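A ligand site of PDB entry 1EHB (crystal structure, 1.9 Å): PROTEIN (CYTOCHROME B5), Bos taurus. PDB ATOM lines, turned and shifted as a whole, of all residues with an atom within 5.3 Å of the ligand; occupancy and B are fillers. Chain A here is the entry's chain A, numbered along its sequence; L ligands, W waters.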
ATOM      1  N   LEU A  21      -5.931 -14.899  16.169  1.00  0.00           N
ATOM      2  CA  LEU A  21      -5.424 -15.263  14.861  1.00  0.00           C
ATOM      3  C   LEU A  21      -6.530 -15.113  13.836  1.00  0.00           C
ATOM      4  O   LEU A  21      -7.708 -15.031  14.194  1.00  0.00           O
ATOM      5  CB  LEU A  21      -4.796 -16.657  14.838  1.00  0.00           C
ATOM      6  CG  LEU A  21      -5.390 -17.865  15.551  1.00  0.00           C
ATOM      7  CD1 LEU A  21      -6.534 -18.437  14.742  1.00  0.00           C
ATOM      8  CD2 LEU A  21      -4.284 -18.900  15.716  1.00  0.00           C
ATOM      9  N   LEU A  23      -8.523 -16.501  10.382  1.00  0.00           N
ATOM     10  CA  LEU A  23      -8.833 -17.658   9.559  1.00  0.00           C
ATOM     11  C   LEU A  23      -9.954 -17.221   8.629  1.00  0.00           C
ATOM     12  O   LEU A  23     -11.035 -16.857   9.089  1.00  0.00           O
ATOM     13  CB  LEU A  23      -9.334 -18.841  10.405  1.00  0.00           C
ATOM     14  CG  LEU A  23      -8.359 -19.515  11.376  1.00  0.00           C
ATOM     15  CD1 LEU A  23      -9.098 -20.616  12.123  1.00  0.00           C
ATOM     16  CD2 LEU A  23      -7.180 -20.102  10.620  1.00  0.00           C
ATOM     17  N   TYR A  28     -10.268 -14.765  15.466  1.00  0.00           N
ATOM     18  CA  TYR A  28     -10.581 -15.681  16.551  1.00  0.00           C
ATOM     19  C   TYR A  28      -9.749 -15.396  17.784  1.00  0.00           C
ATOM     20  O   TYR A  28      -8.546 -15.115  17.673  1.00  0.00           O
ATOM     21  CB  TYR A  28     -10.307 -17.128  16.130  1.00  0.00           C
ATOM     22  CG  TYR A  28     -11.122 -17.614  14.949  1.00  0.00           C
ATOM     23  CD1 TYR A  28     -10.888 -17.122  13.671  1.00  0.00           C
ATOM     24  CD2 TYR A  28     -12.133 -18.564  15.119  1.00  0.00           C
ATOM     25  CE1 TYR A  28     -11.632 -17.561  12.592  1.00  0.00           C
ATOM     26  CE2 TYR A  28     -12.898 -19.007  14.036  1.00  0.00           C
ATOM     27  CZ  TYR A  28     -12.640 -18.493  12.776  1.00  0.00           C
ATOM     28  OH  TYR A  28     -13.396 -18.897  11.690  1.00  0.00           O
ATOM     29  N   LEU A  30      -8.306 -17.230  20.641  1.00  0.00           N
ATOM     30  CA  LEU A  30      -8.074 -18.590  21.100  1.00  0.00           C
ATOM     31  C   LEU A  30      -7.364 -18.698  22.455  1.00  0.00           C
ATOM     32  O   LEU A  30      -6.931 -19.777  22.849  1.00  0.00           O
ATOM     33  CB  LEU A  30      -7.262 -19.352  20.048  1.00  0.00           C
ATOM     34  CG  LEU A  30      -7.913 -19.440  18.671  1.00  0.00           C
ATOM     35  CD1 LEU A  30      -7.056 -20.325  17.771  1.00  0.00           C
ATOM     36  CD2 LEU A  30      -9.315 -20.024  18.792  1.00  0.00           C
ATOM     37  N   PHE A  33      -8.455 -21.507  24.543  1.00  0.00           N
ATOM     38  CA  PHE A  33      -8.514 -22.780  23.817  1.00  0.00           C
ATOM     39  C   PHE A  33      -7.144 -23.446  23.675  1.00  0.00           C
ATOM     40  O   PHE A  33      -7.036 -24.645  23.399  1.00  0.00           O
ATOM     41  CB  PHE A  33      -9.124 -22.531  22.429  1.00  0.00           C
ATOM     42  CG  PHE A  33      -9.263 -23.772  21.581  1.00  0.00           C
ATOM     43  CD1 PHE A  33      -8.547 -23.893  20.399  1.00  0.00           C
ATOM     44  CD2 PHE A  33     -10.130 -24.791  21.949  1.00  0.00           C
ATOM     45  CE1 PHE A  33      -8.695 -25.024  19.578  1.00  0.00           C
ATOM     46  CE2 PHE A  33     -10.288 -25.912  21.148  1.00  0.00           C
ATOM     47  CZ  PHE A  33      -9.570 -26.033  19.956  1.00  0.00           C
ATOM     48  N   HIS A  37      -6.721 -27.539  22.662  1.00  0.00           N
ATOM     49  CA  HIS A  37      -6.484 -27.868  21.264  1.00  0.00           C
ATOM     50  C   HIS A  37      -5.784 -29.217  21.095  1.00  0.00           C
ATOM     51  O   HIS A  37      -4.664 -29.403  21.543  1.00  0.00           O
ATOM     52  CB  HIS A  37      -5.627 -26.773  20.629  1.00  0.00           C
ATOM     53  CG  HIS A  37      -5.388 -26.956  19.172  1.00  0.00           C
ATOM     54  ND1 HIS A  37      -4.162 -26.761  18.569  1.00  0.00           N
ATOM     55  CD2 HIS A  37      -6.242 -27.293  18.173  1.00  0.00           C
ATOM     56  CE1 HIS A  37      -4.321 -26.968  17.256  1.00  0.00           C
ATOM     57  NE2 HIS A  37      -5.568 -27.298  16.972  1.00  0.00           N
ATOM     58  N   PRO A  38      -6.449 -30.180  20.418  1.00  0.00           N
ATOM     59  CA  PRO A  38      -5.852 -31.508  20.205  1.00  0.00           C
ATOM     60  C   PRO A  38      -4.500 -31.445  19.499  1.00  0.00           C
ATOM     61  O   PRO A  38      -3.647 -32.314  19.690  1.00  0.00           O
ATOM     62  CB  PRO A  38      -6.904 -32.229  19.367  1.00  0.00           C
ATOM     63  CG  PRO A  38      -8.185 -31.634  19.882  1.00  0.00           C
ATOM     64  CD  PRO A  38      -7.844 -30.157  19.940  1.00  0.00           C
ATOM     65  N   GLY A  39      -4.309 -30.410  18.690  1.00  0.00           N
ATOM     66  CA  GLY A  39      -3.048 -30.262  17.972  1.00  0.00           C
ATOM     67  C   GLY A  39      -1.963 -29.586  18.788  1.00  0.00           C
ATOM     68  O   GLY A  39      -0.853 -29.377  18.300  1.00  0.00           O
ATOM     69  N   VAL A  43       1.535 -24.987  18.132  1.00  0.00           N
ATOM     70  CA  VAL A  43       1.183 -24.651  16.761  1.00  0.00           C
ATOM     71  C   VAL A  43       0.295 -23.407  16.665  1.00  0.00           C
ATOM     72  O   VAL A  43       0.275 -22.713  15.643  1.00  0.00           O
ATOM     73  CB  VAL A  43       0.479 -25.864  16.078  1.00  0.00           C
ATOM     74  CG1 VAL A  43      -0.793 -26.222  16.812  1.00  0.00           C
ATOM     75  CG2 VAL A  43       0.203 -25.560  14.622  1.00  0.00           C
ATOM     76  N   LEU A  44      -0.436 -23.105  17.740  1.00  0.00           N
ATOM     77  CA  LEU A  44      -1.306 -21.940  17.758  1.00  0.00           C
ATOM     78  C   LEU A  44      -0.505 -20.681  18.104  1.00  0.00           C
ATOM     79  O   LEU A  44      -0.667 -19.636  17.474  1.00  0.00           O
ATOM     80  CB  LEU A  44      -2.441 -22.141  18.766  1.00  0.00           C
ATOM     81  CG  LEU A  44      -3.409 -23.279  18.420  1.00  0.00           C
ATOM     82  CD1 LEU A  44      -4.505 -23.374  19.482  1.00  0.00           C
ATOM     83  CD2 LEU A  44      -4.029 -23.021  17.052  1.00  0.00           C
ATOM     84  N   GLN A  47       1.412 -19.018  15.255  1.00  0.00           N
ATOM     85  CA  GLN A  47       0.638 -18.241  14.283  1.00  0.00           C
ATOM     86  C   GLN A  47      -0.075 -17.050  14.896  1.00  0.00           C
ATOM     87  O   GLN A  47      -0.702 -16.253  14.189  1.00  0.00           O
ATOM     88  CB  GLN A  47      -0.397 -19.154  13.603  1.00  0.00           C
ATOM     89  CG  GLN A  47       0.187 -20.345  12.865  1.00  0.00           C
ATOM     90  CD  GLN A  47       1.136 -19.937  11.755  1.00  0.00           C
ATOM     91  OE1 GLN A  47       0.819 -19.082  10.935  1.00  0.00           O
ATOM     92  NE2 GLN A  47       2.305 -20.570  11.719  1.00  0.00           N
ATOM     93  N   ALA A  52      -3.575 -17.484   9.738  1.00  0.00           N
ATOM     94  CA  ALA A  52      -3.174 -18.898   9.755  1.00  0.00           C
ATOM     95  C   ALA A  52      -4.052 -19.775   8.881  1.00  0.00           C
ATOM     96  O   ALA A  52      -4.055 -20.999   9.013  1.00  0.00           O
ATOM     97  CB  ALA A  52      -3.215 -19.409  11.185  1.00  0.00           C
ATOM     98  N   ASN A  55      -2.240 -22.775   6.973  1.00  0.00           N
ATOM     99  CA  ASN A  55      -1.795 -23.831   7.876  1.00  0.00           C
ATOM    100  C   ASN A  55      -2.986 -24.603   8.404  1.00  0.00           C
ATOM    101  O   ASN A  55      -2.924 -25.814   8.611  1.00  0.00           O
ATOM    102  CB  ASN A  55      -1.005 -23.241   9.038  1.00  0.00           C
ATOM    103  CG  ASN A  55      -0.085 -22.118   8.614  1.00  0.00           C
ATOM    104  OD1 ASN A  55      -0.551 -21.060   8.200  1.00  0.00           O
ATOM    105  ND2 ASN A  55       1.217 -22.355   8.693  1.00  0.00           N
ATOM    106  N   PHE A  56      -4.076 -23.889   8.631  1.00  0.00           N
ATOM    107  CA  PHE A  56      -5.309 -24.461   9.142  1.00  0.00           C
ATOM    108  C   PHE A  56      -5.905 -25.446   8.134  1.00  0.00           C
ATOM    109  O   PHE A  56      -6.333 -26.541   8.503  1.00  0.00           O
ATOM    110  CB  PHE A  56      -6.320 -23.348   9.426  1.00  0.00           C
ATOM    111  CG  PHE A  56      -7.638 -23.833   9.957  1.00  0.00           C
ATOM    112  CD1 PHE A  56      -7.740 -24.276  11.265  1.00  0.00           C
ATOM    113  CD2 PHE A  56      -8.765 -23.825   9.151  1.00  0.00           C
ATOM    114  CE1 PHE A  56      -8.964 -24.733  11.765  1.00  0.00           C
ATOM    115  CE2 PHE A  56      -9.996 -24.276   9.631  1.00  0.00           C
ATOM    116  CZ  PHE A  56     -10.092 -24.733  10.948  1.00  0.00           C
ATOM    117  N   VAL A  59      -3.741 -28.823   7.274  1.00  0.00           N
ATOM    118  CA  VAL A  59      -3.887 -29.975   8.154  1.00  0.00           C
ATOM    119  C   VAL A  59      -5.249 -30.623   7.922  1.00  0.00           C
ATOM    120  O   VAL A  59      -5.497 -31.748   8.358  1.00  0.00           O
ATOM    121  CB  VAL A  59      -3.772 -29.561   9.635  1.00  0.00           C
ATOM    122  CG1 VAL A  59      -2.407 -28.930   9.895  1.00  0.00           C
ATOM    123  CG2 VAL A  59      -4.852 -28.579   9.969  1.00  0.00           C
ATOM    124  N   GLY A  60      -6.136 -29.900   7.241  1.00  0.00           N
ATOM    125  CA  GLY A  60      -7.467 -30.416   6.943  1.00  0.00           C
ATOM    126  C   GLY A  60      -8.364 -30.743   8.115  1.00  0.00           C
ATOM    127  O   GLY A  60      -8.734 -31.901   8.319  1.00  0.00           O
ATOM    128  N   HIS A  61      -8.716 -29.725   8.896  1.00  0.00           N
ATOM    129  CA  HIS A  61      -9.587 -29.911  10.064  1.00  0.00           C
ATOM    130  C   HIS A  61     -10.941 -30.505   9.709  1.00  0.00           C
ATOM    131  O   HIS A  61     -11.487 -30.250   8.641  1.00  0.00           O
ATOM    132  CB  HIS A  61      -9.803 -28.578  10.784  1.00  0.00           C
ATOM    133  CG  HIS A  61      -8.632 -28.148  11.595  1.00  0.00           C
ATOM    134  ND1 HIS A  61      -7.477 -27.608  11.066  1.00  0.00           N
ATOM    135  CD2 HIS A  61      -8.429 -28.215  12.933  1.00  0.00           C
ATOM    136  CE1 HIS A  61      -6.631 -27.378  12.087  1.00  0.00           C
ATOM    137  NE2 HIS A  61      -7.168 -27.736  13.233  1.00  0.00           N
ATOM    138  N   SER A  62     -11.473 -31.300  10.632  1.00  0.00           N
ATOM    139  CA  SER A  62     -12.762 -31.964  10.451  1.00  0.00           C
ATOM    140  C   SER A  62     -13.932 -30.993  10.573  1.00  0.00           C
ATOM    141  O   SER A  62     -13.770 -29.849  10.988  1.00  0.00           O
ATOM    142  CB  SER A  62     -12.920 -33.073  11.500  1.00  0.00           C
ATOM    143  OG  SER A  62     -13.006 -32.517  12.796  1.00  0.00           O
ATOM    144  N   ALA A  65     -14.516 -29.790  14.115  1.00  0.00           N
ATOM    145  CA  ALA A  65     -13.528 -28.793  14.524  1.00  0.00           C
ATOM    146  C   ALA A  65     -13.906 -27.422  14.011  1.00  0.00           C
ATOM    147  O   ALA A  65     -13.765 -26.425  14.718  1.00  0.00           O
ATOM    148  CB  ALA A  65     -12.154 -29.178  14.007  1.00  0.00           C
ATOM    149  N   LEU A  68     -16.884 -26.003  15.869  1.00  0.00           N
ATOM    150  CA  LEU A  68     -16.458 -25.552  17.184  1.00  0.00           C
ATOM    151  C   LEU A  68     -15.747 -24.203  17.119  1.00  0.00           C
ATOM    152  O   LEU A  68     -15.902 -23.377  18.015  1.00  0.00           O
ATOM    153  CB  LEU A  68     -15.516 -26.589  17.814  1.00  0.00           C
ATOM    154  CG  LEU A  68     -14.852 -26.180  19.132  1.00  0.00           C
ATOM    155  CD1 LEU A  68     -15.911 -25.916  20.185  1.00  0.00           C
ATOM    156  CD2 LEU A  68     -13.904 -27.280  19.599  1.00  0.00           C
ATOM    157  N   SER A  69     -14.966 -23.989  16.064  1.00  0.00           N
ATOM    158  CA  SER A  69     -14.218 -22.745  15.906  1.00  0.00           C
ATOM    159  C   SER A  69     -15.079 -21.499  15.928  1.00  0.00           C
ATOM    160  O   SER A  69     -14.655 -20.443  16.395  1.00  0.00           O
ATOM    161  CB  SER A  69     -13.411 -22.777  14.590  1.00  0.00           C
ATOM    162  OG  SER A  69     -14.240 -22.614  13.459  1.00  0.00           O
ATOM    163  N   PHE A  72     -15.375 -19.086  18.882  1.00  0.00           N
ATOM    164  CA  PHE A  72     -14.261 -18.199  19.232  1.00  0.00           C
ATOM    165  C   PHE A  72     -14.142 -16.940  18.365  1.00  0.00           C
ATOM    166  O   PHE A  72     -13.213 -16.136  18.548  1.00  0.00           O
ATOM    167  CB  PHE A  72     -12.954 -18.995  19.183  1.00  0.00           C
ATOM    168  CG  PHE A  72     -12.931 -20.186  20.126  1.00  0.00           C
ATOM    169  CD1 PHE A  72     -12.992 -19.995  21.501  1.00  0.00           C
ATOM    170  CD2 PHE A  72     -12.869 -21.476  19.622  1.00  0.00           C
ATOM    171  CE1 PHE A  72     -13.000 -21.094  22.382  1.00  0.00           C
ATOM    172  CE2 PHE A  72     -12.867 -22.584  20.483  1.00  0.00           C
ATOM    173  CZ  PHE A  72     -12.936 -22.382  21.869  1.00  0.00           C
HETATM  174  C1  LIG L   1      -6.061 -30.931  15.323  1.00  0.00           C
HETATM  175  C2  LIG L   1      -9.599 -27.836  16.491  1.00  0.00           C
HETATM  176  C3  LIG L   1      -6.930 -24.183  14.775  1.00  0.00           C
HETATM  177  C4  LIG L   1      -3.266 -27.254  13.878  1.00  0.00           C
HETATM  178  C5  LIG L   1      -7.277 -30.397  15.706  1.00  0.00           C
HETATM  179  C6  LIG L   1      -8.425 -31.186  16.114  1.00  0.00           C
HETATM  180  C7  LIG L   1      -9.376 -30.317  16.513  1.00  0.00           C
HETATM  181  C8  LIG L   1      -8.847 -28.984  16.302  1.00  0.00           C
HETATM  182  C9  LIG L   1     -10.729 -30.637  17.147  1.00  0.00           C
HETATM  183  C10 LIG L   1      -8.573 -32.705  16.001  1.00  0.00           C
HETATM  184  C11 LIG L   1      -8.718 -33.216  14.570  1.00  0.00           C
HETATM  185  C12 LIG L   1      -9.911 -32.618  13.858  1.00  0.00           C
HETATM  186  O1  LIG L   1     -11.023 -32.672  14.411  1.00  0.00           O
HETATM  187  O2  LIG L   1      -9.733 -32.103  12.738  1.00  0.00           O
HETATM  188  C13 LIG L   1      -9.171 -26.575  16.118  1.00  0.00           C
HETATM  189  C14 LIG L   1      -9.983 -25.370  16.245  1.00  0.00           C
HETATM  190  C15 LIG L   1      -9.227 -24.344  15.859  1.00  0.00           C
HETATM  191  C16 LIG L   1      -7.960 -24.899  15.369  1.00  0.00           C
HETATM  192  C17 LIG L   1     -11.424 -25.276  16.725  1.00  0.00           C
HETATM  193  C18 LIG L   1      -9.561 -23.019  16.117  1.00  0.00           C
HETATM  194  C19 LIG L   1      -9.749 -22.057  15.140  1.00  0.00           C
HETATM  195  C20 LIG L   1      -5.723 -24.711  14.320  1.00  0.00           C
HETATM  196  C21 LIG L   1      -4.683 -23.935  13.675  1.00  0.00           C
HETATM  197  C22 LIG L   1      -3.634 -24.776  13.451  1.00  0.00           C
HETATM  198  C23 LIG L   1      -4.028 -26.082  13.956  1.00  0.00           C
HETATM  199  C24 LIG L   1      -4.753 -22.446  13.336  1.00  0.00           C
HETATM  200  C25 LIG L   1      -2.454 -24.513  12.769  1.00  0.00           C
HETATM  201  C26 LIG L   1      -1.688 -23.349  12.889  1.00  0.00           C
HETATM  202  C27 LIG L   1      -3.706 -28.539  14.224  1.00  0.00           C
HETATM  203  C28 LIG L   1      -2.898 -29.774  14.154  1.00  0.00           C
HETATM  204  C29 LIG L   1      -3.694 -30.807  14.511  1.00  0.00           C
HETATM  205  C30 LIG L   1      -4.983 -30.208  14.851  1.00  0.00           C
HETATM  206  C31 LIG L   1      -1.425 -29.872  13.813  1.00  0.00           C
HETATM  207  C32 LIG L   1      -3.353 -32.311  14.575  1.00  0.00           C
HETATM  208  C33 LIG L   1      -3.380 -32.985  13.211  1.00  0.00           C
HETATM  209  C34 LIG L   1      -2.822 -34.391  13.224  1.00  0.00           C
HETATM  210  O3  LIG L   1      -2.103 -34.759  12.281  1.00  0.00           O
HETATM  211  O4  LIG L   1      -3.100 -35.145  14.186  1.00  0.00           O
HETATM  212  N1  LIG L   1      -7.566 -29.034  15.771  1.00  0.00           N
HETATM  213  N2  LIG L   1      -7.929 -26.288  15.563  1.00  0.00           N
HETATM  214  N3  LIG L   1      -5.339 -26.041  14.460  1.00  0.00           N
HETATM  215  N4  LIG L   1      -4.976 -28.813  14.695  1.00  0.00           N
HETATM  216 FE1  LIG L   1      -6.445 -27.545  15.121  1.00  0.00          FE
HETATM  217  O   HOH W   1     -11.798 -34.756  16.062  1.00  0.00           O
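FE1 of the ligand is bound by NE2 of His 61 (2.0 Å).
NE2 of His 37 is bound to FE1 of the ligand (2.1 Å).
An oxygen (O2) of the ligand sits at hydrogen-bond distance from the backbone NH (N) of Ser 62 (2.8 Å).
The side-chain hydroxyl of Ser 62 sits at hydrogen-bond distance from an oxygen (O1) of the ligand.
The side-chain hydroxyl (OG) of Ser 62 lies within hydrogen-bond range of the backbone NH (N) of Ala 65.
ND1 of His 61 is in hydrogen-bond range of O of Phe 56 (3.0 Å).
CD1 of Leu 23 touches C19 of the ligand, at 3.4 Å.
CE1 of Phe 33 touches C14 of the ligand (3.6 Å).
CB of Pro 38 touches C6 of the ligand (3.7 Å).
Gly 39 touches the ligand.
CG2 of Val 43 touches C26 of the ligand, 3.4 Å away.
Leu 44 touches the ligand (CD2 to C21, 3.6 Å).
Gln 47 touches the ligand.
Asn 55 touches the ligand (CB to C26, 3.9 Å).
Phe 56 touches the ligand (CD1 to C3, 3.6 Å).
O of Ala 65 touches C17 of the ligand (3.3 Å).
Ser 69 touches the ligand.
Hydrophobic or aromatic side chains within 4 Å of the ligand: Leu 23, Phe 33, His 37, Pro 38, Val 43, Leu 44, Phe 56, His 61 and Ala 65.
Of the 22 residues printed, 14 come within 4 Å of the ligand.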
